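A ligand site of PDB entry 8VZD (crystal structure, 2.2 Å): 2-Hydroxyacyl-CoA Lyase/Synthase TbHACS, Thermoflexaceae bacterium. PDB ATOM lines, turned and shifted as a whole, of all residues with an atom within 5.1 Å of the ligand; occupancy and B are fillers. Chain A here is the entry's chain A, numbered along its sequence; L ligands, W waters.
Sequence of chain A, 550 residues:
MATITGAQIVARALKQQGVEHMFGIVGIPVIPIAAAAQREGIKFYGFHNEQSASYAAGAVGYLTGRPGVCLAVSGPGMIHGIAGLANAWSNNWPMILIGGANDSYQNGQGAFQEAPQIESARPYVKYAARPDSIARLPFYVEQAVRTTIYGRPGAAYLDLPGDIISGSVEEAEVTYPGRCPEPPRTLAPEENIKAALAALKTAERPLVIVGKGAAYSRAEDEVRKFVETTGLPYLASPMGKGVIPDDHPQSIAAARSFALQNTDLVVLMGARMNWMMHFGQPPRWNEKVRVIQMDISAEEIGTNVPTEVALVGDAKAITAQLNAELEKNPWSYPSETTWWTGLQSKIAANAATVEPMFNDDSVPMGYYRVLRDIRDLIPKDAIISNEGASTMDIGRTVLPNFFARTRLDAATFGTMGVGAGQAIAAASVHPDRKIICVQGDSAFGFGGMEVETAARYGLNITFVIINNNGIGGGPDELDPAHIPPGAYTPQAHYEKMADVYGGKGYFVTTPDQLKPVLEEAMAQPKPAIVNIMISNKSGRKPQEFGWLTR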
ATOM      1  N   ASN A  91      -0.686   6.216  13.086  1.00  0.00           N
ATOM      2  CA  ASN A  91       0.481   6.229  12.215  1.00  0.00           C
ATOM      3  C   ASN A  91       0.191   6.770  10.818  1.00  0.00           C
ATOM      4  O   ASN A  91       1.110   6.821   9.996  1.00  0.00           O
ATOM      5  CB  ASN A  91       1.054   4.814  12.106  1.00  0.00           C
ATOM      6  CG  ASN A  91       1.677   4.340  13.395  1.00  0.00           C
ATOM      7  OD1 ASN A  91       2.728   4.837  13.796  1.00  0.00           O
ATOM      8  ND2 ASN A  91       1.046   3.376  14.044  1.00  0.00           N
ATOM      9  N   ASN A  92      -1.050   7.159  10.546  1.00  0.00           N
ATOM     10  CA  ASN A  92      -1.455   7.625   9.224  1.00  0.00           C
ATOM     11  C   ASN A  92      -1.131   6.583   8.151  1.00  0.00           C
ATOM     12  O   ASN A  92      -0.444   6.859   7.166  1.00  0.00           O
ATOM     13  CB  ASN A  92      -0.821   8.977   8.885  1.00  0.00           C
ATOM     14  CG  ASN A  92      -1.123  10.039   9.916  1.00  0.00           C
ATOM     15  OD1 ASN A  92      -2.269  10.472  10.065  1.00  0.00           O
ATOM     16  ND2 ASN A  92      -0.104  10.475  10.645  1.00  0.00           N
ATOM     17  N   ARG A 152      -3.587  12.966   3.642  1.00  0.00           N
ATOM     18  CA  ARG A 152      -2.921  12.280   4.734  1.00  0.00           C
ATOM     19  C   ARG A 152      -3.524  10.885   4.868  1.00  0.00           C
ATOM     20  O   ARG A 152      -4.719  10.772   5.196  1.00  0.00           O
ATOM     21  CB  ARG A 152      -3.077  13.053   6.044  1.00  0.00           C
ATOM     22  CG  ARG A 152      -2.103  12.611   7.129  1.00  0.00           C
ATOM     23  CD  ARG A 152      -2.291  13.397   8.416  1.00  0.00           C
ATOM     24  NE  ARG A 152      -1.065  13.436   9.214  1.00  0.00           N
ATOM     25  CZ  ARG A 152      -0.955  14.062  10.377  1.00  0.00           C
ATOM     26  NH1 ARG A 152      -1.977  14.697  10.920  1.00  0.00           N
ATOM     27  NH2 ARG A 152       0.212  14.053  10.998  1.00  0.00           N
ATOM     28  N   PRO A 153      -2.772   9.815   4.606  1.00  0.00           N
ATOM     29  CA  PRO A 153      -3.370   8.478   4.603  1.00  0.00           C
ATOM     30  C   PRO A 153      -3.946   8.105   5.954  1.00  0.00           C
ATOM     31  O   PRO A 153      -3.484   8.560   7.006  1.00  0.00           O
ATOM     32  CB  PRO A 153      -2.209   7.557   4.206  1.00  0.00           C
ATOM     33  CG  PRO A 153      -0.976   8.357   4.489  1.00  0.00           C
ATOM     34  CD  PRO A 153      -1.338   9.794   4.280  1.00  0.00           C
ATOM     35  N   GLY A 211      12.082  10.436   8.924  1.00  0.00           N
ATOM     36  CA  GLY A 211      10.995   9.701   9.534  1.00  0.00           C
ATOM     37  C   GLY A 211      10.364   8.696   8.578  1.00  0.00           C
ATOM     38  O   GLY A 211      10.736   8.581   7.414  1.00  0.00           O
ATOM     39  N   LYS A 212       9.397   7.955   9.102  1.00  0.00           N
ATOM     40  CA  LYS A 212       8.718   6.939   8.296  1.00  0.00           C
ATOM     41  C   LYS A 212       7.713   7.532   7.325  1.00  0.00           C
ATOM     42  O   LYS A 212       7.154   6.795   6.512  1.00  0.00           O
ATOM     43  CB  LYS A 212       8.036   5.903   9.194  1.00  0.00           C
ATOM     44  CG  LYS A 212       6.810   6.388   9.958  1.00  0.00           C
ATOM     45  CD  LYS A 212       6.102   5.208  10.609  1.00  0.00           C
ATOM     46  CE  LYS A 212       4.826   5.620  11.329  1.00  0.00           C
ATOM     47  NZ  LYS A 212       5.106   6.357  12.596  1.00  0.00           N
ATOM     48  N   GLY A 213       7.475   8.846   7.395  1.00  0.00           N
ATOM     49  CA  GLY A 213       6.712   9.498   6.334  1.00  0.00           C
ATOM     50  C   GLY A 213       7.483   9.549   5.034  1.00  0.00           C
ATOM     51  O   GLY A 213       6.908   9.400   3.955  1.00  0.00           O
ATOM     52  N   TYR A 216       7.247   5.995   3.744  1.00  0.00           N
ATOM     53  CA  TYR A 216       5.961   5.724   3.110  1.00  0.00           C
ATOM     54  C   TYR A 216       5.877   6.351   1.721  1.00  0.00           C
ATOM     55  O   TYR A 216       5.258   5.779   0.818  1.00  0.00           O
ATOM     56  CB  TYR A 216       4.817   6.217   3.987  1.00  0.00           C
ATOM     57  CG  TYR A 216       3.449   6.039   3.370  1.00  0.00           C
ATOM     58  CD1 TYR A 216       2.778   4.823   3.473  1.00  0.00           C
ATOM     59  CD2 TYR A 216       2.829   7.069   2.675  1.00  0.00           C
ATOM     60  CE1 TYR A 216       1.531   4.645   2.900  1.00  0.00           C
ATOM     61  CE2 TYR A 216       1.584   6.903   2.101  1.00  0.00           C
ATOM     62  CZ  TYR A 216       0.941   5.684   2.224  1.00  0.00           C
ATOM     63  OH  TYR A 216      -0.304   5.519   1.650  1.00  0.00           O
ATOM     64  N   SER A 217       6.497   7.512   1.542  1.00  0.00           N
ATOM     65  CA  SER A 217       6.469   8.187   0.250  1.00  0.00           C
ATOM     66  C   SER A 217       7.396   7.561  -0.770  1.00  0.00           C
ATOM     67  O   SER A 217       7.490   8.073  -1.890  1.00  0.00           O
ATOM     68  CB  SER A 217       6.819   9.664   0.441  1.00  0.00           C
ATOM     69  OG  SER A 217       6.829  10.358  -0.802  1.00  0.00           O
ATOM     70  N   SER A 237      14.474   8.132  12.521  1.00  0.00           N
ATOM     71  CA  SER A 237      13.421   7.757  13.445  1.00  0.00           C
ATOM     72  C   SER A 237      13.393   6.241  13.580  1.00  0.00           C
ATOM     73  O   SER A 237      14.008   5.538  12.770  1.00  0.00           O
ATOM     74  CB  SER A 237      12.082   8.307  12.961  1.00  0.00           C
ATOM     75  OG  SER A 237      11.625   7.594  11.827  1.00  0.00           O
ATOM     76  N   MET A 239      11.261   3.856  12.789  1.00  0.00           N
ATOM     77  CA  MET A 239      10.916   3.221  11.519  1.00  0.00           C
ATOM     78  C   MET A 239      11.420   3.996  10.313  1.00  0.00           C
ATOM     79  O   MET A 239      11.238   3.543   9.179  1.00  0.00           O
ATOM     80  CB  MET A 239       9.397   3.014  11.424  1.00  0.00           C
ATOM     81  CG  MET A 239       8.895   1.918  12.354  1.00  0.00           C
ATOM     82  SD  MET A 239       7.137   1.562  12.197  1.00  0.00           S
ATOM     83  CE  MET A 239       7.044   1.044  10.490  1.00  0.00           C
ATOM     84  N   GLY A 240      12.060   5.151  10.538  1.00  0.00           N
ATOM     85  CA  GLY A 240      12.831   5.794   9.485  1.00  0.00           C
ATOM     86  C   GLY A 240      14.146   5.104   9.189  1.00  0.00           C
ATOM     87  O   GLY A 240      14.783   5.440   8.176  1.00  0.00           O
ATOM     88  N   GLY A 270       9.381  13.972   6.873  1.00  0.00           N
ATOM     89  CA  GLY A 270       8.369  12.970   7.173  1.00  0.00           C
ATOM     90  C   GLY A 270       8.399  12.468   8.597  1.00  0.00           C
ATOM     91  O   GLY A 270       8.246  11.267   8.835  1.00  0.00           O
ATOM     92  N   ALA A 271       8.587  13.370   9.561  1.00  0.00           N
ATOM     93  CA  ALA A 271       8.611  13.006  10.970  1.00  0.00           C
ATOM     94  C   ALA A 271       7.939  14.114  11.774  1.00  0.00           C
ATOM     95  O   ALA A 271       8.127  15.294  11.480  1.00  0.00           O
ATOM     96  CB  ALA A 271      10.038  12.766  11.474  1.00  0.00           C
ATOM     97  N   ARG A 272       7.174  13.719  12.780  1.00  0.00           N
ATOM     98  CA  ARG A 272       6.408  14.659  13.590  1.00  0.00           C
ATOM     99  C   ARG A 272       7.167  15.033  14.860  1.00  0.00           C
ATOM    100  O   ARG A 272       7.984  14.260  15.363  1.00  0.00           O
ATOM    101  CB  ARG A 272       5.049  14.076  13.953  1.00  0.00           C
ATOM    102  CG  ARG A 272       4.073  13.995  12.795  1.00  0.00           C
ATOM    103  CD  ARG A 272       2.756  13.351  13.217  1.00  0.00           C
ATOM    104  NE  ARG A 272       2.901  11.923  13.458  1.00  0.00           N
ATOM    105  CZ  ARG A 272       1.901  11.108  13.758  1.00  0.00           C
ATOM    106  NH1 ARG A 272       0.659  11.560  13.881  1.00  0.00           N
ATOM    107  NH2 ARG A 272       2.145   9.818  13.937  1.00  0.00           N
ATOM    108  N   ASN A 274       6.164  14.907  17.822  1.00  0.00           N
ATOM    109  CA  ASN A 274       5.284  14.358  18.851  1.00  0.00           C
ATOM    110  C   ASN A 274       6.103  13.791  20.016  1.00  0.00           C
ATOM    111  O   ASN A 274       7.197  14.287  20.297  1.00  0.00           O
ATOM    112  CB  ASN A 274       4.375  13.271  18.258  1.00  0.00           C
ATOM    113  CG  ASN A 274       5.151  12.173  17.567  1.00  0.00           C
ATOM    114  OD1 ASN A 274       6.377  12.147  17.587  1.00  0.00           O
ATOM    115  ND2 ASN A 274       4.424  11.245  16.941  1.00  0.00           N
ATOM    116  N   MET A 276       7.712  11.061  20.224  1.00  0.00           N
ATOM    117  CA  MET A 276       8.948  10.412  19.800  1.00  0.00           C
ATOM    118  C   MET A 276      10.104  11.408  19.757  1.00  0.00           C
ATOM    119  O   MET A 276      11.235  11.067  20.121  1.00  0.00           O
ATOM    120  CB  MET A 276       8.766   9.739  18.448  1.00  0.00           C
ATOM    121  CG  MET A 276       8.007   8.435  18.487  1.00  0.00           C
ATOM    122  SD  MET A 276       8.241   7.471  16.989  1.00  0.00           S
ATOM    123  CE  MET A 276       7.270   6.017  17.370  1.00  0.00           C
ATOM    124  N   MET A 277       9.840  12.637  19.302  1.00  0.00           N
ATOM    125  CA  MET A 277      10.848  13.680  19.249  1.00  0.00           C
ATOM    126  C   MET A 277      10.771  14.620  20.442  1.00  0.00           C
ATOM    127  O   MET A 277      11.340  15.719  20.400  1.00  0.00           O
ATOM    128  CB  MET A 277      10.734  14.453  17.943  1.00  0.00           C
ATOM    129  CG  MET A 277      10.977  13.601  16.705  1.00  0.00           C
ATOM    130  SD  MET A 277      12.637  12.872  16.716  1.00  0.00           S
ATOM    131  CE  MET A 277      12.457  11.604  15.460  1.00  0.00           C
ATOM    132  N   MET A 294       8.901  19.161   6.632  1.00  0.00           N
ATOM    133  CA  MET A 294       8.415  18.582   5.382  1.00  0.00           C
ATOM    134  C   MET A 294       7.348  17.538   5.725  1.00  0.00           C
ATOM    135  O   MET A 294       7.667  16.490   6.293  1.00  0.00           O
ATOM    136  CB  MET A 294       9.567  17.950   4.591  1.00  0.00           C
ATOM    137  CG  MET A 294       9.138  17.260   3.315  1.00  0.00           C
ATOM    138  SD  MET A 294      10.488  16.319   2.564  1.00  0.00           S
ATOM    139  CE  MET A 294      11.743  17.582   2.435  1.00  0.00           C
ATOM    140  N   ASP A 295       6.105  17.832   5.373  1.00  0.00           N
ATOM    141  CA  ASP A 295       4.995  16.952   5.716  1.00  0.00           C
ATOM    142  C   ASP A 295       3.863  17.126   4.716  1.00  0.00           C
ATOM    143  O   ASP A 295       3.640  18.230   4.196  1.00  0.00           O
ATOM    144  CB  ASP A 295       4.492  17.233   7.139  1.00  0.00           C
ATOM    145  CG  ASP A 295       3.684  16.076   7.724  1.00  0.00           C
ATOM    146  OD1 ASP A 295       2.698  15.649   7.086  1.00  0.00           O
ATOM    147  OD2 ASP A 295       4.061  15.586   8.816  1.00  0.00           O
ATOM    148  N   ILE A 296       3.160  16.031   4.432  1.00  0.00           N
ATOM    149  CA  ILE A 296       2.034  16.087   3.505  1.00  0.00           C
ATOM    150  C   ILE A 296       0.820  16.733   4.161  1.00  0.00           C
ATOM    151  O   ILE A 296      -0.069  17.233   3.465  1.00  0.00           O
ATOM    152  CB  ILE A 296       1.688  14.677   2.984  1.00  0.00           C
ATOM    153  CG1 ILE A 296       0.818  14.758   1.731  1.00  0.00           C
ATOM    154  CG2 ILE A 296       0.993  13.859   4.069  1.00  0.00           C
ATOM    155  CD1 ILE A 296       0.464  13.395   1.154  1.00  0.00           C
ATOM    156  N   SER A 297       0.774  16.757   5.496  1.00  0.00           N
ATOM    157  CA  SER A 297      -0.356  17.312   6.236  1.00  0.00           C
ATOM    158  C   SER A 297      -0.024  18.755   6.611  1.00  0.00           C
ATOM    159  O   SER A 297       0.861  18.996   7.428  1.00  0.00           O
ATOM    160  CB  SER A 297      -0.643  16.477   7.475  1.00  0.00           C
ATOM    161  OG  SER A 297      -1.627  17.087   8.284  1.00  0.00           O
ATOM    162  N   GLU A 300      -0.275  19.599  10.316  1.00  0.00           N
ATOM    163  CA  GLU A 300       0.821  19.194  11.189  1.00  0.00           C
ATOM    164  C   GLU A 300       1.889  20.265  11.326  1.00  0.00           C
ATOM    165  O   GLU A 300       2.645  20.254  12.307  1.00  0.00           O
ATOM    166  CB  GLU A 300       1.448  17.893  10.676  1.00  0.00           C
ATOM    167  CG  GLU A 300       2.425  17.234  11.644  1.00  0.00           C
ATOM    168  CD  GLU A 300       1.777  16.821  12.948  1.00  0.00           C
ATOM    169  OE1 GLU A 300       0.663  16.258  12.894  1.00  0.00           O
ATOM    170  OE2 GLU A 300       2.379  17.058  14.017  1.00  0.00           O
ATOM    171  N   GLY A 313       3.759  18.929   1.255  1.00  0.00           N
ATOM    172  CA  GLY A 313       3.587  18.138   0.058  1.00  0.00           C
ATOM    173  C   GLY A 313       4.204  16.763   0.217  1.00  0.00           C
ATOM    174  O   GLY A 313       4.464  16.309   1.332  1.00  0.00           O
ATOM    175  N   ASP A 314       4.443  16.112  -0.922  1.00  0.00           N
ATOM    176  CA  ASP A 314       4.998  14.769  -0.939  1.00  0.00           C
ATOM    177  C   ASP A 314       6.504  14.819  -0.696  1.00  0.00           C
ATOM    178  O   ASP A 314       7.216  15.642  -1.268  1.00  0.00           O
ATOM    179  CB  ASP A 314       4.699  14.095  -2.273  1.00  0.00           C
ATOM    180  CG  ASP A 314       5.297  12.698  -2.364  1.00  0.00           C
ATOM    181  OD1 ASP A 314       4.793  11.798  -1.667  1.00  0.00           O
ATOM    182  OD2 ASP A 314       6.265  12.526  -3.130  1.00  0.00           O
ATOM    183  N   ALA A 315       6.980  13.895   0.144  1.00  0.00           N
ATOM    184  CA  ALA A 315       8.388  13.902   0.529  1.00  0.00           C
ATOM    185  C   ALA A 315       9.297  13.648  -0.663  1.00  0.00           C
ATOM    186  O   ALA A 315      10.318  14.326  -0.836  1.00  0.00           O
ATOM    187  CB  ALA A 315       8.646  12.871   1.626  1.00  0.00           C
ATOM    188  N   THR A 412       3.911   4.734  16.390  1.00  0.00           N
ATOM    189  CA  THR A 412       3.524   5.932  17.133  1.00  0.00           C
ATOM    190  C   THR A 412       2.599   5.611  18.296  1.00  0.00           C
ATOM    191  O   THR A 412       2.679   6.240  19.357  1.00  0.00           O
ATOM    192  CB  THR A 412       2.853   6.933  16.187  1.00  0.00           C
ATOM    193  OG1 THR A 412       3.703   7.149  15.042  1.00  0.00           O
ATOM    194  CG2 THR A 412       2.628   8.264  16.890  1.00  0.00           C
HETATM  195  P1  LIG L   1       8.120   8.977  12.795  1.00  0.00           P
HETATM  196  O1  LIG L   1       7.276   8.181  13.762  1.00  0.00           O
HETATM  197  O2  LIG L   1       9.034   8.138  11.939  1.00  0.00           O
HETATM  198  O3  LIG L   1       8.771  10.210  13.385  1.00  0.00           O
HETATM  199  P2  LIG L   1       5.603  10.070  12.175  1.00  0.00           P
HETATM  200  O4  LIG L   1       4.623   8.948  11.945  1.00  0.00           O
HETATM  201  O5  LIG L   1       5.668  10.740  13.533  1.00  0.00           O
HETATM  202  O6  LIG L   1       7.062   9.573  11.741  1.00  0.00           O
HETATM  203  O7  LIG L   1       5.325  11.207  11.076  1.00  0.00           O
HETATM  204  C1  LIG L   1       5.041  10.827   9.729  1.00  0.00           C
HETATM  205  C2  LIG L   1       4.537  12.042   8.967  1.00  0.00           C
HETATM  206  O8  LIG L   1       4.766  11.876   7.563  1.00  0.00           O
HETATM  207  C3  LIG L   1       3.041  12.245   9.160  1.00  0.00           C
HETATM  208  O9  LIG L   1       2.819  13.461   9.876  1.00  0.00           O
HETATM  209  C4  LIG L   1       2.459  12.350   7.772  1.00  0.00           C
HETATM  210  O10 LIG L   1       1.624  13.511   7.669  1.00  0.00           O
HETATM  211  C5  LIG L   1       3.677  12.485   6.859  1.00  0.00           C
HETATM  212  N1  LIG L   1       3.459  11.852   5.532  1.00  0.00           N
HETATM  213  C6  LIG L   1       2.676  10.791   5.262  1.00  0.00           C
HETATM  214  N2  LIG L   1       2.714  10.501   3.936  1.00  0.00           N
HETATM  215  C7  LIG L   1       3.537  11.392   3.341  1.00  0.00           C
HETATM  216  C8  LIG L   1       4.017  11.653   1.968  1.00  0.00           C
HETATM  217  N3  LIG L   1       3.624  10.884   0.923  1.00  0.00           N
HETATM  218  N4  LIG L   1       4.870  12.688   1.791  1.00  0.00           N
HETATM  219  C9  LIG L   1       5.273  13.460   2.816  1.00  0.00           C
HETATM  220  N5  LIG L   1       4.867  13.281   4.081  1.00  0.00           N
HETATM  221  C10 LIG L   1       4.021  12.280   4.406  1.00  0.00           C
HETATM  222  O   HOH W   1       2.328   9.144  10.031  1.00  0.00           O
HETATM  223  O   HOH W   2       0.908   9.736   0.109  1.00  0.00           O
HETATM  224  O   HOH W   3       8.050  11.481  15.609  1.00  0.00           O
HETATM  225  O   HOH W   4       5.710   9.020  15.534  1.00  0.00           O
HETATM  226  O   HOH W   5       8.561   5.692  13.833  1.00  0.00           O
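The backbone NH (N) of Arg 272 lies close to an oxygen (O5) of the ligand (3.4 Å).
A nitrogen (N5) of the ligand lies within hydrogen-bond range of the backbone NH of Ile 296, at 3.3 Å.
OG of Ser 237 is in hydrogen-bond range of O2 of the ligand (2.6 Å).
N of Lys 212 sits at hydrogen-bond distance from O2 of the ligand (2.9 Å).
An oxygen (O10) of the ligand is in hydrogen-bond range of the side-chain carboxylate (OD1) of Asp 295 (2.5 Å).
The side-chain carboxylate of Asp 314 sits at hydrogen-bond distance from a nitrogen (N3) of the ligand.
An oxygen (O9) of the ligand is in hydrogen-bond range of the guanidinium group of Arg 152.
An oxygen (O4) of the ligand is in salt-bridge range of the side-chain amino group of Lys 212 (2.7 Å).
O5 of the ligand lies within salt-bridge range of NE of Arg 272 (3.0 Å).
N of Ala 315 lies within hydrogen-bond range of N4 of the ligand, 2.9 Å away.
The side-chain sulfur of Met 276 lies close to an oxygen (O1) of the ligand, 3.4 Å away.
ND2 of Asn 92 touches C3 of the ligand, at 3.9 Å.
CA of Gly 211 touches O2 of the ligand, 3.5 Å away.
Gly 213 touches the ligand (CA to O8, 3.3 Å).
Tyr 216 touches the ligand (CD2 to N2, 3.7 Å).
Ser 217 touches the ligand (CB to N3, 3.5 Å).
Gly 270 touches the ligand (O to C1, 3.4 Å).
CB of Ala 271 touches O3 of the ligand, 3.4 Å away.
ND2 of Asn 274 touches O5 of the ligand, at 3.7 Å.
Ser 297 touches the ligand.
Gly 313 touches the ligand (O to C9, 3.3 Å).
Thr 412 touches the ligand.
Hydrophobic or aromatic side chains that line the ligand: Tyr 216, Ala 271, Met 276, Ile 296 and Ala 315.
Within 4 Å of the ligand: Asn 92, Arg 152, Gly 211, Lys 212, Gly 213, Tyr 216, Ser 217, Ser 237, Gly 270, Ala 271, Arg 272, Asn 274, Met 276, Asp 295, Ile 296, Ser 297, Gly 313, Asp 314, Ala 315 and Thr 412.
Along chain A the residues within 4 Å of the ligand span positions 92 to 412.
The nearest printed residue that does not touch the ligand is Pro 153 (4.1 Å).
The side-chain amide oxygen (OD1) of Asn 91 sits at hydrogen-bond distance from the side-chain amino group (NZ) of Lys 212 (3.1 Å).
NE of Arg 152 is in hydrogen-bond range of OD1 of Asn 92 (3.3 Å).
O of Gly 270 sits at hydrogen-bond distance from N of Gly 213 (2.9 Å).
OG1 of Thr 412 sits at hydrogen-bond distance from NH2 of Arg 272, at 3.3 Å.
The side-chain carboxylate of Asp 295 lies within hydrogen-bond range of the backbone NH of Ser 297, 2.7 Å away.
The guanidinium group (NH1) of Arg 272 lies close to the side-chain amide nitrogen (ND2) of Asn 92.
N of Ile 296 lies close to O of Gly 313.
N of Gly 240 is in hydrogen-bond range of OG of Ser 237.
Water W4 lies within hydrogen-bond range of an oxygen (O1) of the ligand (2.5 Å), the side-chain hydroxyl of Thr 412 (2.8 Å), the side-chain amide nitrogen of Asn 274 (2.9 Å) and the side-chain sulfur of Met 276 (3.3 Å).
Water W3 lies within hydrogen-bond range of an oxygen (O3) of the ligand (2.7 Å), the side-chain amide oxygen (OD1) of Asn 274 (2.7 Å) and the backbone carbonyl oxygen (O) of Arg 272 (2.8 Å).
Water W5 lies within hydrogen-bond range of O1 of the ligand (2.8 Å), N of Met 239 (3.4 Å) and SD of Met 276 (3.6 Å).
Water W1 lies within hydrogen-bond range of O of Asn 91 (2.6 Å), ND2 of Asn 92 (2.8 Å) and O4 of the ligand (3.0 Å).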
